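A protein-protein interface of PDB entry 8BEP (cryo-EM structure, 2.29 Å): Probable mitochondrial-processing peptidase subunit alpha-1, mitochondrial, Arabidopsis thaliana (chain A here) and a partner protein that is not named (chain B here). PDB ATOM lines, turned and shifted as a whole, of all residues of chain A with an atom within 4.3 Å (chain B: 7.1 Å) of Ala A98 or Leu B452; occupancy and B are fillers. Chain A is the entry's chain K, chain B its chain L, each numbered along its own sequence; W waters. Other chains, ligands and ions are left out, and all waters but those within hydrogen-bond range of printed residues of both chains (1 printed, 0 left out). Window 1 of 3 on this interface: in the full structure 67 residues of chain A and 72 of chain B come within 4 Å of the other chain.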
ATOM      1  N   THR A  94      -3.213   5.693   3.707  1.00  0.00           N
ATOM      2  CA  THR A  94      -3.594   6.977   3.134  1.00  0.00           C
ATOM      3  C   THR A  94      -4.254   7.812   4.216  1.00  0.00           C
ATOM      4  O   THR A  94      -4.811   7.241   5.163  1.00  0.00           O
ATOM      5  CB  THR A  94      -4.543   6.815   1.939  1.00  0.00           C
ATOM      6  OG1 THR A  94      -4.681   8.070   1.265  1.00  0.00           O
ATOM      7  CG2 THR A  94      -5.915   6.371   2.396  1.00  0.00           C
ATOM      8  N   ASN A  96      -6.886   9.588   3.689  1.00  0.00           N
ATOM      9  CA  ASN A  96      -8.308   9.600   3.375  1.00  0.00           C
ATOM     10  C   ASN A  96      -9.048   8.573   4.232  1.00  0.00           C
ATOM     11  O   ASN A  96      -8.579   7.442   4.387  1.00  0.00           O
ATOM     12  CB  ASN A  96      -8.504   9.303   1.885  1.00  0.00           C
ATOM     13  CG  ASN A  96      -9.855   8.685   1.561  1.00  0.00           C
ATOM     14  OD1 ASN A  96     -10.893   9.091   2.082  1.00  0.00           O
ATOM     15  ND2 ASN A  96      -9.842   7.687   0.685  1.00  0.00           N
ATOM     16  N   PRO A  97     -10.207   8.928   4.794  1.00  0.00           N
ATOM     17  CA  PRO A  97     -10.959   7.965   5.619  1.00  0.00           C
ATOM     18  C   PRO A  97     -11.472   6.741   4.870  1.00  0.00           C
ATOM     19  O   PRO A  97     -11.873   5.771   5.521  1.00  0.00           O
ATOM     20  CB  PRO A  97     -12.123   8.811   6.156  1.00  0.00           C
ATOM     21  CG  PRO A  97     -12.214   9.968   5.206  1.00  0.00           C
ATOM     22  CD  PRO A  97     -10.794  10.273   4.881  1.00  0.00           C
ATOM     23  N   ALA A  98     -11.584   6.742   3.561  1.00  0.00           N
ATOM     24  CA  ALA A  98     -11.999   5.543   2.797  1.00  0.00           C
ATOM     25  C   ALA A  98     -10.902   4.499   2.530  1.00  0.00           C
ATOM     26  O   ALA A  98      -9.777   4.848   2.295  1.00  0.00           O
ATOM     27  CB  ALA A  98     -12.641   5.877   1.514  1.00  0.00           C
ATOM     28  N   ALA A  99     -11.298   3.249   2.550  1.00  0.00           N
ATOM     29  CA  ALA A  99     -10.397   2.107   2.294  1.00  0.00           C
ATOM     30  C   ALA A  99     -10.921   1.360   1.076  1.00  0.00           C
ATOM     31  O   ALA A  99     -12.095   1.382   0.852  1.00  0.00           O
ATOM     32  CB  ALA A  99     -10.260   1.224   3.509  1.00  0.00           C
ATOM     33  N   ASN A 149     -19.513  -1.051  -0.650  1.00  0.00           N
ATOM     34  CA  ASN A 149     -19.834  -1.333  -2.040  1.00  0.00           C
ATOM     35  C   ASN A 149     -18.894  -2.412  -2.552  1.00  0.00           C
ATOM     36  O   ASN A 149     -17.693  -2.377  -2.277  1.00  0.00           O
ATOM     37  CB  ASN A 149     -19.711  -0.078  -2.913  1.00  0.00           C
ATOM     38  CG  ASN A 149     -20.539   1.073  -2.393  1.00  0.00           C
ATOM     39  OD1 ASN A 149     -20.027   1.962  -1.715  1.00  0.00           O
ATOM     40  ND2 ASN A 149     -21.828   1.059  -2.700  1.00  0.00           N
ATOM     41  N   ASP A 164     -15.164  -1.525  -1.116  1.00  0.00           N
ATOM     42  CA  ASP A 164     -14.859  -0.130  -0.664  1.00  0.00           C
ATOM     43  C   ASP A 164     -15.731   0.233   0.537  1.00  0.00           C
ATOM     44  O   ASP A 164     -16.885  -0.008   0.499  1.00  0.00           O
ATOM     45  CB  ASP A 164     -15.099   0.899  -1.769  1.00  0.00           C
ATOM     46  CG  ASP A 164     -14.369   0.724  -3.087  1.00  0.00           C
ATOM     47  OD1 ASP A 164     -13.390  -0.017  -3.140  1.00  0.00           O
ATOM     48  OD2 ASP A 164     -14.801   1.369  -4.062  1.00  0.00           O
ATOM     49  N   ALA A 165     -15.133   0.767   1.574  1.00  0.00           N
ATOM     50  CA  ALA A 165     -15.849   1.194   2.770  1.00  0.00           C
ATOM     51  C   ALA A 165     -14.946   2.123   3.573  1.00  0.00           C
ATOM     52  O   ALA A 165     -13.801   2.385   3.202  1.00  0.00           O
ATOM     53  CB  ALA A 165     -16.301  -0.004   3.613  1.00  0.00           C
ATOM     54  N   LEU A 166     -15.479   2.618   4.685  1.00  0.00           N
ATOM     55  CA  LEU A 166     -14.694   3.422   5.606  1.00  0.00           C
ATOM     56  C   LEU A 166     -13.610   2.573   6.266  1.00  0.00           C
ATOM     57  O   LEU A 166     -13.737   1.354   6.396  1.00  0.00           O
ATOM     58  CB  LEU A 166     -15.599   4.052   6.663  1.00  0.00           C
ATOM     59  CG  LEU A 166     -16.510   5.185   6.183  1.00  0.00           C
ATOM     60  CD1 LEU A 166     -17.077   5.958   7.358  1.00  0.00           C
ATOM     61  CD2 LEU A 166     -15.766   6.117   5.235  1.00  0.00           C
ATOM     62  N   LYS A 167     -12.536   3.243   6.693  1.00  0.00           N
ATOM     63  CA  LYS A 167     -11.340   2.540   7.146  1.00  0.00           C
ATOM     64  C   LYS A 167     -11.565   1.782   8.448  1.00  0.00           C
ATOM     65  O   LYS A 167     -10.807   0.860   8.763  1.00  0.00           O
ATOM     66  CB  LYS A 167     -10.191   3.531   7.317  1.00  0.00           C
ATOM     67  CG  LYS A 167      -9.429   3.790   6.044  1.00  0.00           C
ATOM     68  CD  LYS A 167      -8.467   4.965   6.167  1.00  0.00           C
ATOM     69  CE  LYS A 167      -8.279   5.430   7.592  1.00  0.00           C
ATOM     70  NZ  LYS A 167      -7.328   6.568   7.648  1.00  0.00           N
ATOM     71  N   SER A 263      -5.690  -0.260  -0.265  1.00  0.00           N
ATOM     72  CA  SER A 263      -5.313   1.171  -0.119  1.00  0.00           C
ATOM     73  C   SER A 263      -6.137   1.744   1.023  1.00  0.00           C
ATOM     74  O   SER A 263      -7.354   1.698   0.919  1.00  0.00           O
ATOM     75  CB  SER A 263      -5.491   1.940  -1.313  1.00  0.00           C
ATOM     76  OG  SER A 263      -4.880   3.204  -1.158  1.00  0.00           O
ATOM     77  N   GLY A 264      -5.500   2.184   2.084  1.00  0.00           N
ATOM     78  CA  GLY A 264      -6.207   2.893   3.162  1.00  0.00           C
ATOM     79  C   GLY A 264      -6.158   2.128   4.436  1.00  0.00           C
ATOM     80  O   GLY A 264      -6.952   2.343   5.320  1.00  0.00           O
ATOM     81  N   ARG A 434      -8.722   6.648  -5.195  1.00  0.00           N
ATOM     82  CA  ARG A 434      -8.204   5.551  -4.326  1.00  0.00           C
ATOM     83  C   ARG A 434      -8.456   4.185  -4.984  1.00  0.00           C
ATOM     84  O   ARG A 434      -7.571   3.312  -4.878  1.00  0.00           O
ATOM     85  CB  ARG A 434      -8.857   5.662  -2.944  1.00  0.00           C
ATOM     86  CG  ARG A 434      -9.027   4.344  -2.202  1.00  0.00           C
ATOM     87  CD  ARG A 434     -10.049   4.495  -1.093  1.00  0.00           C
ATOM     88  NE  ARG A 434     -11.255   5.170  -1.554  1.00  0.00           N
ATOM     89  CZ  ARG A 434     -12.371   4.561  -1.937  1.00  0.00           C
ATOM     90  NH1 ARG A 434     -12.453   3.243  -1.908  1.00  0.00           N
ATOM     91  NH2 ARG A 434     -13.408   5.275  -2.339  1.00  0.00           N
ATOM     92  N   ILE B  91     -10.792   9.162  12.339  1.00  0.00           N
ATOM     93  CA  ILE B  91     -10.505   9.015  10.919  1.00  0.00           C
ATOM     94  C   ILE B  91     -11.109  10.131  10.079  1.00  0.00           C
ATOM     95  O   ILE B  91     -10.890  10.166   8.866  1.00  0.00           O
ATOM     96  CB  ILE B  91     -11.007   7.650  10.407  1.00  0.00           C
ATOM     97  CG1 ILE B  91     -12.524   7.678  10.209  1.00  0.00           C
ATOM     98  CG2 ILE B  91     -10.619   6.547  11.369  1.00  0.00           C
ATOM     99  CD1 ILE B  91     -13.054   6.543   9.371  1.00  0.00           C
ATOM    100  N   LEU B 446     -25.454   6.538   4.037  1.00  0.00           N
ATOM    101  CA  LEU B 446     -25.320   7.927   3.614  1.00  0.00           C
ATOM    102  C   LEU B 446     -23.968   8.503   4.013  1.00  0.00           C
ATOM    103  O   LEU B 446     -23.317   9.172   3.206  1.00  0.00           O
ATOM    104  CB  LEU B 446     -26.458   8.773   4.192  1.00  0.00           C
ATOM    105  CG  LEU B 446     -26.372  10.282   3.940  1.00  0.00           C
ATOM    106  CD1 LEU B 446     -26.416  10.586   2.444  1.00  0.00           C
ATOM    107  CD2 LEU B 446     -27.472  11.027   4.679  1.00  0.00           C
ATOM    108  N   LYS B 447     -23.529   8.253   5.249  1.00  0.00           N
ATOM    109  CA  LYS B 447     -22.207   8.716   5.668  1.00  0.00           C
ATOM    110  C   LYS B 447     -21.119   8.137   4.773  1.00  0.00           C
ATOM    111  O   LYS B 447     -20.231   8.862   4.293  1.00  0.00           O
ATOM    112  CB  LYS B 447     -21.953   8.329   7.123  1.00  0.00           C
ATOM    113  CG  LYS B 447     -22.895   8.951   8.122  1.00  0.00           C
ATOM    114  CD  LYS B 447     -22.268   8.996   9.493  1.00  0.00           C
ATOM    115  CE  LYS B 447     -22.856   7.930  10.398  1.00  0.00           C
ATOM    116  NZ  LYS B 447     -22.650   8.243  11.837  1.00  0.00           N
ATOM    117  N   SER B 448     -21.190   6.829   4.517  1.00  0.00           N
ATOM    118  CA  SER B 448     -20.175   6.191   3.693  1.00  0.00           C
ATOM    119  C   SER B 448     -20.185   6.744   2.274  1.00  0.00           C
ATOM    120  O   SER B 448     -19.124   6.971   1.688  1.00  0.00           O
ATOM    121  CB  SER B 448     -20.379   4.678   3.687  1.00  0.00           C
ATOM    122  OG  SER B 448     -19.431   4.043   2.856  1.00  0.00           O
ATOM    123  N   SER B 449     -21.369   6.966   1.703  1.00  0.00           N
ATOM    124  CA  SER B 449     -21.441   7.455   0.331  1.00  0.00           C
ATOM    125  C   SER B 449     -21.003   8.909   0.229  1.00  0.00           C
ATOM    126  O   SER B 449     -20.455   9.316  -0.800  1.00  0.00           O
ATOM    127  CB  SER B 449     -22.854   7.278  -0.221  1.00  0.00           C
ATOM    128  OG  SER B 449     -23.753   8.214   0.337  1.00  0.00           O
ATOM    129  N   LEU B 450     -21.236   9.704   1.275  1.00  0.00           N
ATOM    130  CA  LEU B 450     -20.747  11.075   1.272  1.00  0.00           C
ATOM    131  C   LEU B 450     -19.232  11.122   1.374  1.00  0.00           C
ATOM    132  O   LEU B 450     -18.602  12.015   0.798  1.00  0.00           O
ATOM    133  CB  LEU B 450     -21.385  11.872   2.410  1.00  0.00           C
ATOM    134  CG  LEU B 450     -22.872  12.197   2.251  1.00  0.00           C
ATOM    135  CD1 LEU B 450     -23.441  12.819   3.516  1.00  0.00           C
ATOM    136  CD2 LEU B 450     -23.100  13.100   1.056  1.00  0.00           C
ATOM    137  N   LEU B 451     -18.628  10.125   2.029  1.00  0.00           N
ATOM    138  CA  LEU B 451     -17.155  10.150   2.254  1.00  0.00           C
ATOM    139  C   LEU B 451     -16.406   9.395   1.146  1.00  0.00           C
ATOM    140  O   LEU B 451     -15.200   9.658   0.981  1.00  0.00           O
ATOM    141  CB  LEU B 451     -16.874   9.530   3.625  1.00  0.00           C
ATOM    142  CG  LEU B 451     -15.851  10.273   4.480  1.00  0.00           C
ATOM    143  CD1 LEU B 451     -16.049  11.778   4.380  1.00  0.00           C
ATOM    144  CD2 LEU B 451     -15.932   9.819   5.927  1.00  0.00           C
ATOM    145  N   LEU B 452     -17.081   8.497   0.424  1.00  0.00           N
ATOM    146  CA  LEU B 452     -16.434   7.697  -0.610  1.00  0.00           C
ATOM    147  C   LEU B 452     -16.342   8.414  -1.947  1.00  0.00           C
ATOM    148  O   LEU B 452     -15.369   8.216  -2.682  1.00  0.00           O
ATOM    149  CB  LEU B 452     -17.184   6.376  -0.804  1.00  0.00           C
ATOM    150  CG  LEU B 452     -16.569   5.111  -0.200  1.00  0.00           C
ATOM    151  CD1 LEU B 452     -16.102   5.353   1.222  1.00  0.00           C
ATOM    152  CD2 LEU B 452     -17.552   3.952  -0.249  1.00  0.00           C
ATOM    153  N   HIS B 453     -17.327   9.254  -2.291  1.00  0.00           N
ATOM    154  CA  HIS B 453     -17.254  10.037  -3.561  1.00  0.00           C
ATOM    155  C   HIS B 453     -16.254  11.190  -3.415  1.00  0.00           C
ATOM    156  O   HIS B 453     -16.013  11.888  -4.421  1.00  0.00           O
ATOM    157  CB  HIS B 453     -18.648  10.529  -3.985  1.00  0.00           C
ATOM    158  CG  HIS B 453     -19.041  11.847  -3.406  1.00  0.00           C
ATOM    159  ND1 HIS B 453     -19.560  11.972  -2.132  1.00  0.00           N
ATOM    160  CD2 HIS B 453     -19.009  13.095  -3.924  1.00  0.00           C
ATOM    161  CE1 HIS B 453     -19.822  13.240  -1.889  1.00  0.00           C
ATOM    162  NE2 HIS B 453     -19.491  13.949  -2.971  1.00  0.00           N
ATOM    163  N   MET B 454     -15.675  11.362  -2.229  1.00  0.00           N
ATOM    164  CA  MET B 454     -14.754  12.457  -1.933  1.00  0.00           C
ATOM    165  C   MET B 454     -13.303  12.120  -2.269  1.00  0.00           C
ATOM    166  O   MET B 454     -12.417  12.326  -1.445  1.00  0.00           O
ATOM    167  CB  MET B 454     -14.882  12.807  -0.457  1.00  0.00           C
ATOM    168  CG  MET B 454     -14.940  14.258  -0.151  1.00  0.00           C
ATOM    169  SD  MET B 454     -16.106  15.150  -1.167  1.00  0.00           S
ATOM    170  CE  MET B 454     -15.871  16.731  -0.407  1.00  0.00           C
ATOM    171  N   ASP B 455     -13.021  11.630  -3.473  1.00  0.00           N
ATOM    172  CA  ASP B 455     -11.645  11.322  -3.847  1.00  0.00           C
ATOM    173  C   ASP B 455     -11.335  11.924  -5.207  1.00  0.00           C
ATOM    174  O   ASP B 455     -12.116  11.779  -6.152  1.00  0.00           O
ATOM    175  CB  ASP B 455     -11.378   9.808  -3.850  1.00  0.00           C
ATOM    176  CG  ASP B 455     -12.354   9.039  -4.709  1.00  0.00           C
ATOM    177  OD1 ASP B 455     -13.438   9.577  -5.012  1.00  0.00           O
ATOM    178  OD2 ASP B 455     -12.033   7.888  -5.077  1.00  0.00           O
HETATM  179  O   HOH W   1     -18.461   2.557   5.125  1.00  0.00           O
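Water W1 lies within hydrogen-bond range of the side-chain hydroxyl of Ser B448 and the backbone NH of Leu A166.
Printed residues of chain B within 4 Å of Pro A97: Ile B91 and Leu B451. Of chain B, only Leu B452 (3.5 Å) comes within 4 Å of Ala A98. Of the printed residues of chain B, Leu A166 touches Leu B451 (3.8 Å). Ser A263 touches none of the printed residues of chain B. Of the printed residues of chain A, Ile B91 touches Pro A97 (3.3 Å). Leu B450 touches none of the printed residues of chain A. Of the printed residues of chain A, Leu B451 touches Pro A97 (3.7 Å) and Leu A166 (3.8 Å). Of the printed residues of chain A, Leu B452 touches Ala A98 (3.5 Å), Asn A149 (3.5 Å) and Arg A434 (3.6 Å). The nearest printed residue of chain B that does not touch Arg A434 is His B453 (5.6 Å).
Of the 13 printed residues of chain A, 5 touch a printed residue of chain B. Printed residues of chain A that touch a printed residue of chain B: Pro A97, Ala A98, Asn A149, Leu A166 and Arg A434. Of the 11 printed residues of chain B, 4 touch a printed residue of chain A. Among the printed residues, no Asp or Glu carboxylate lies within 4 Å of a Lys or Arg side-chain nitrogen of the other chain.
CB of Pro A97 touches O of Ile B91, 3.3 Å away. Pro A97 touches Leu B451 (CG to CG, 3.7 Å). Ala A98 touches Leu B452 (CB to CD1, 3.5 Å). CD2 of Leu B452 touches OD1 of Asn A149, 3.5 Å away. Leu A166 touches Leu B451. Arg A434 touches Leu B452. Arg A434 touches Asp B455.
O of Asn A149 lies within hydrogen-bond range of N of Asp A164 (2.9 Å). The side-chain amide oxygen (OD1) of Asn A96 is in hydrogen-bond range of the backbone NH (N) of Ala A98 (2.9 Å). OD1 of Asp A164 lies within salt-bridge range of NH1 of Arg A434 (3.6 Å). O of Ala A99 sits at hydrogen-bond distance from NH1 of Arg A434. O of Pro A97 sits at hydrogen-bond distance from N of Lys A167, at 2.9 Å.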
